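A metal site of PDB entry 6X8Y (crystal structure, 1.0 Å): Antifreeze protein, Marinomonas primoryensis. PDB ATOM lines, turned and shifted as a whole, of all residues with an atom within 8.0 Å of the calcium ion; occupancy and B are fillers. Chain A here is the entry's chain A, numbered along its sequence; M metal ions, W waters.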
ATOM      1  N   TYR A  15      19.405  33.620  -8.717  1.00  0.00           N
ATOM      2  CA  TYR A  15      20.136  32.448  -9.176  1.00  0.00           C
ATOM      3  C   TYR A  15      19.986  32.314 -10.691  1.00  0.00           C
ATOM      4  O   TYR A  15      18.891  32.491 -11.220  1.00  0.00           O
ATOM      5  CB  TYR A  15      19.564  31.164  -8.494  1.00  0.00           C
ATOM      6  CG  TYR A  15      20.090  29.919  -9.149  1.00  0.00           C
ATOM      7  CD1 TYR A  15      21.395  29.455  -8.859  1.00  0.00           C
ATOM      8  CD2 TYR A  15      19.343  29.239 -10.100  1.00  0.00           C
ATOM      9  CE1 TYR A  15      21.905  28.337  -9.527  1.00  0.00           C
ATOM     10  CE2 TYR A  15      19.865  28.122 -10.760  1.00  0.00           C
ATOM     11  CZ  TYR A  15      21.129  27.671 -10.461  1.00  0.00           C
ATOM     12  OH  TYR A  15      21.679  26.598 -11.116  1.00  0.00           O
ATOM     13  N   VAL A  55      26.143  22.446  -8.267  1.00  0.00           N
ATOM     14  CA  VAL A  55      25.090  23.216  -7.556  1.00  0.00           C
ATOM     15  C   VAL A  55      23.814  23.310  -8.407  1.00  0.00           C
ATOM     16  O   VAL A  55      22.729  23.458  -7.835  1.00  0.00           O
ATOM     17  CB  VAL A  55      25.567  24.648  -7.199  1.00  0.00           C
ATOM     18  CG1 VAL A  55      25.480  25.651  -8.349  1.00  0.00           C
ATOM     19  CG2 VAL A  55      24.802  25.166  -5.978  1.00  0.00           C
ATOM     20  N   ALA A  56      23.945  23.236  -9.736  1.00  0.00           N
ATOM     21  CA  ALA A  56      22.830  23.503 -10.640  1.00  0.00           C
ATOM     22  C   ALA A  56      21.974  22.268 -10.918  1.00  0.00           C
ATOM     23  O   ALA A  56      20.961  22.390 -11.631  1.00  0.00           O
ATOM     24  CB  ALA A  56      23.369  24.108 -11.929  1.00  0.00           C
ATOM     25  N   LYS A  57      22.331  21.129 -10.330  1.00  0.00           N
ATOM     26  CA  LYS A  57      21.575  19.891 -10.565  1.00  0.00           C
ATOM     27  C   LYS A  57      20.636  19.580  -9.392  1.00  0.00           C
ATOM     28  O   LYS A  57      20.968  19.889  -8.218  1.00  0.00           O
ATOM     29  CB  LYS A  57      22.568  18.731 -10.767  1.00  0.00           C
ATOM     30  CG  LYS A  57      23.324  18.796 -12.091  1.00  0.00           C
ATOM     31  CD  LYS A  57      22.468  18.582 -13.329  1.00  0.00           C
ATOM     32  CE  LYS A  57      23.166  18.651 -14.680  1.00  0.00           C
ATOM     33  NZ  LYS A  57      23.678  17.331 -15.102  1.00  0.00           N
ATOM     34  N   GLY A  58      19.483  18.979  -9.702  1.00  0.00           N
ATOM     35  CA  GLY A  58      18.604  18.459  -8.665  1.00  0.00           C
ATOM     36  C   GLY A  58      18.235  19.491  -7.625  1.00  0.00           C
ATOM     37  O   GLY A  58      17.868  20.635  -7.930  1.00  0.00           O
ATOM     38  N   THR A  59      18.341  19.081  -6.367  1.00  0.00           N
ATOM     39  CA  THR A  59      18.020  19.941  -5.243  1.00  0.00           C
ATOM     40  C   THR A  59      19.288  20.497  -4.579  1.00  0.00           C
ATOM     41  O   THR A  59      19.240  20.956  -3.421  1.00  0.00           O
ATOM     42  CB  THR A  59      17.165  19.188  -4.208  1.00  0.00           C
ATOM     43  OG1 THR A  59      17.872  18.034  -3.724  1.00  0.00           O
ATOM     44  CG2 THR A  59      15.872  18.710  -4.830  1.00  0.00           C
ATOM     45  N   HIS A  60      20.399  20.500  -5.306  1.00  0.00           N
ATOM     46  CA  HIS A  60      21.651  20.982  -4.712  1.00  0.00           C
ATOM     47  C   HIS A  60      21.595  22.461  -4.362  1.00  0.00           C
ATOM     48  O   HIS A  60      22.196  22.870  -3.347  1.00  0.00           O
ATOM     49  CB  HIS A  60      22.807  20.645  -5.617  1.00  0.00           C
ATOM     50  CG  HIS A  60      22.978  19.170  -5.794  1.00  0.00           C
ATOM     51  ND1 HIS A  60      23.598  18.618  -6.882  1.00  0.00           N
ATOM     52  CD2 HIS A  60      22.546  18.142  -5.025  1.00  0.00           C
ATOM     53  CE1 HIS A  60      23.571  17.298  -6.762  1.00  0.00           C
ATOM     54  NE2 HIS A  60      22.960  16.981  -5.648  1.00  0.00           N
ATOM     55  N   LEU A  61      20.894  23.284  -5.148  1.00  0.00           N
ATOM     56  CA  LEU A  61      20.810  24.711  -4.816  1.00  0.00           C
ATOM     57  C   LEU A  61      20.093  24.896  -3.483  1.00  0.00           C
ATOM     58  O   LEU A  61      20.480  25.716  -2.643  1.00  0.00           O
ATOM     59  CB  LEU A  61      20.091  25.449  -5.923  1.00  0.00           C
ATOM     60  CG  LEU A  61      19.875  26.954  -5.681  1.00  0.00           C
ATOM     61  CD1 LEU A  61      21.196  27.699  -5.600  1.00  0.00           C
ATOM     62  CD2 LEU A  61      18.949  27.546  -6.719  1.00  0.00           C
ATOM     63  N   GLN A  62      18.987  24.169  -3.301  1.00  0.00           N
ATOM     64  CA  GLN A  62      18.242  24.235  -2.045  1.00  0.00           C
ATOM     65  C   GLN A  62      19.141  23.896  -0.874  1.00  0.00           C
ATOM     66  O   GLN A  62      19.113  24.542   0.174  1.00  0.00           O
ATOM     67  CB  GLN A  62      17.067  23.241  -2.095  1.00  0.00           C
ATOM     68  CG  GLN A  62      15.915  23.665  -2.931  1.00  0.00           C
ATOM     69  CD  GLN A  62      16.033  23.462  -4.447  1.00  0.00           C
ATOM     70  OE1 GLN A  62      17.052  23.046  -4.972  1.00  0.00           O
ATOM     71  NE2 GLN A  62      14.962  23.788  -5.154  1.00  0.00           N
ATOM     72  N   LEU A  72      12.933  30.724  -1.989  1.00  0.00           N
ATOM     73  CA  LEU A  72      13.045  30.559  -3.436  1.00  0.00           C
ATOM     74  C   LEU A  72      11.706  30.799  -4.129  1.00  0.00           C
ATOM     75  O   LEU A  72      10.670  30.267  -3.737  1.00  0.00           O
ATOM     76  CB  LEU A  72      13.533  29.164  -3.777  1.00  0.00           C
ATOM     77  CG  LEU A  72      15.045  28.947  -3.654  1.00  0.00           C
ATOM     78  CD1 LEU A  72      15.379  27.457  -3.615  1.00  0.00           C
ATOM     79  CD2 LEU A  72      15.782  29.634  -4.813  1.00  0.00           C
ATOM     80  N   THR A  74      11.019  29.713  -7.144  1.00  0.00           N
ATOM     81  CA  THR A  74      10.759  28.538  -7.952  1.00  0.00           C
ATOM     82  C   THR A  74      11.893  27.564  -7.679  1.00  0.00           C
ATOM     83  O   THR A  74      12.932  27.952  -7.141  1.00  0.00           O
ATOM     84  CB  THR A  74      10.606  28.937  -9.420  1.00  0.00           C
ATOM     85  OG1 THR A  74      10.066  27.854 -10.175  1.00  0.00           O
ATOM     86  CG2 THR A  74      11.929  29.342 -10.002  1.00  0.00           C
ATOM     87  N   ASP A  75      11.705  26.302  -8.088  1.00  0.00           N
ATOM     88  CA  ASP A  75      12.757  25.293  -8.086  1.00  0.00           C
ATOM     89  C   ASP A  75      13.330  25.229  -9.493  1.00  0.00           C
ATOM     90  O   ASP A  75      12.655  24.709 -10.387  1.00  0.00           O
ATOM     91  CB  ASP A  75      12.156  23.933  -7.674  1.00  0.00           C
ATOM     92  CG  ASP A  75      13.153  22.801  -7.717  1.00  0.00           C
ATOM     93  OD1 ASP A  75      14.363  23.067  -7.976  1.00  0.00           O
ATOM     94  OD2 ASP A  75      12.738  21.651  -7.475  1.00  0.00           O
ATOM     95  N   PRO A  76      14.526  25.772  -9.743  1.00  0.00           N
ATOM     96  CA  PRO A  76      15.083  25.709 -11.100  1.00  0.00           C
ATOM     97  C   PRO A  76      15.203  24.282 -11.601  1.00  0.00           C
ATOM     98  O   PRO A  76      15.433  23.338 -10.826  1.00  0.00           O
ATOM     99  CB  PRO A  76      16.485  26.340 -10.939  1.00  0.00           C
ATOM    100  CG  PRO A  76      16.448  27.101  -9.671  1.00  0.00           C
ATOM    101  CD  PRO A  76      15.473  26.388  -8.778  1.00  0.00           C
ATOM    102  N   GLY A  77      15.094  24.130 -12.920  1.00  0.00           N
ATOM    103  CA  GLY A  77      15.447  22.882 -13.545  1.00  0.00           C
ATOM    104  C   GLY A  77      16.963  22.646 -13.529  1.00  0.00           C
ATOM    105  O   GLY A  77      17.744  23.462 -13.051  1.00  0.00           O
ATOM    106  N   ASP A  78      17.380  21.489 -14.053  1.00  0.00           N
ATOM    107  CA  ASP A  78      18.794  21.156 -14.066  1.00  0.00           C
ATOM    108  C   ASP A  78      19.548  22.029 -15.050  1.00  0.00           C
ATOM    109  O   ASP A  78      19.079  22.335 -16.162  1.00  0.00           O
ATOM    110  CB  ASP A  78      18.991  19.712 -14.515  1.00  0.00           C
ATOM    111  CG  ASP A  78      18.658  18.670 -13.487  1.00  0.00           C
ATOM    112  OD1 ASP A  78      18.377  19.003 -12.312  1.00  0.00           O
ATOM    113  OD2 ASP A  78      18.741  17.475 -13.850  1.00  0.00           O
ATOM    114  N   ASN A  79      20.775  22.360 -14.661  1.00  0.00           N
ATOM    115  CA  ASN A  79      21.778  22.918 -15.556  1.00  0.00           C
ATOM    116  C   ASN A  79      23.130  22.347 -15.148  1.00  0.00           C
ATOM    117  O   ASN A  79      23.254  21.767 -14.067  1.00  0.00           O
ATOM    118  CB  ASN A  79      21.852  24.455 -15.446  1.00  0.00           C
ATOM    119  CG  ASN A  79      20.757  25.168 -16.191  1.00  0.00           C
ATOM    120  OD1 ASN A  79      19.929  25.842 -15.580  1.00  0.00           O
ATOM    121  ND2 ASN A  79      20.784  25.098 -17.505  1.00  0.00           N
HETATM  122 CA    CA M   1      16.252  21.942  -9.132  1.00  0.00          CA
HETATM  123  O   HOH W   1      18.217  22.658 -10.363  1.00  0.00           O
HETATM  124  O   HOH W   2      14.889  20.248  -8.222  1.00  0.00           O
HETATM  125  O   HOH W   3      17.392  23.534  -7.677  1.00  0.00           O
HETATM  126  O   HOH W   4      16.318  20.305 -10.865  1.00  0.00           O
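OD1 of Asp 78 sits at hydrogen-bond distance from N of Gly 58 (2.8 Å).
OD1 of Asp 75 sits close to NE2 of Gln 62, 3.0 Å away.
Three residues have an atom within 4 Å of the calcium ion: Gly 58, Asp 75 and Pro 76.
The nearest printed residue that does not touch the calcium ion is Gln 62 (4.4 Å).
The calcium ion is bound by O of Pro 76 (2.3 Å).
Water W2 binds the calcium ion (2.4 Å).
The calcium ion is bound by water W4 (2.4 Å).
The calcium ion is bound by O of Gly 58 (2.4 Å).
The calcium ion is bound by water W1 (2.4 Å).
The calcium ion is bound by water W3 (2.4 Å).
OD1 of Asp 75 binds the calcium ion (2.5 Å).
The calcium ion has seven donor atoms within binding distance.
Water W1 bridges the backbone carbonyl oxygen of Gly 77 and the backbone carbonyl oxygen of Ala 56.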
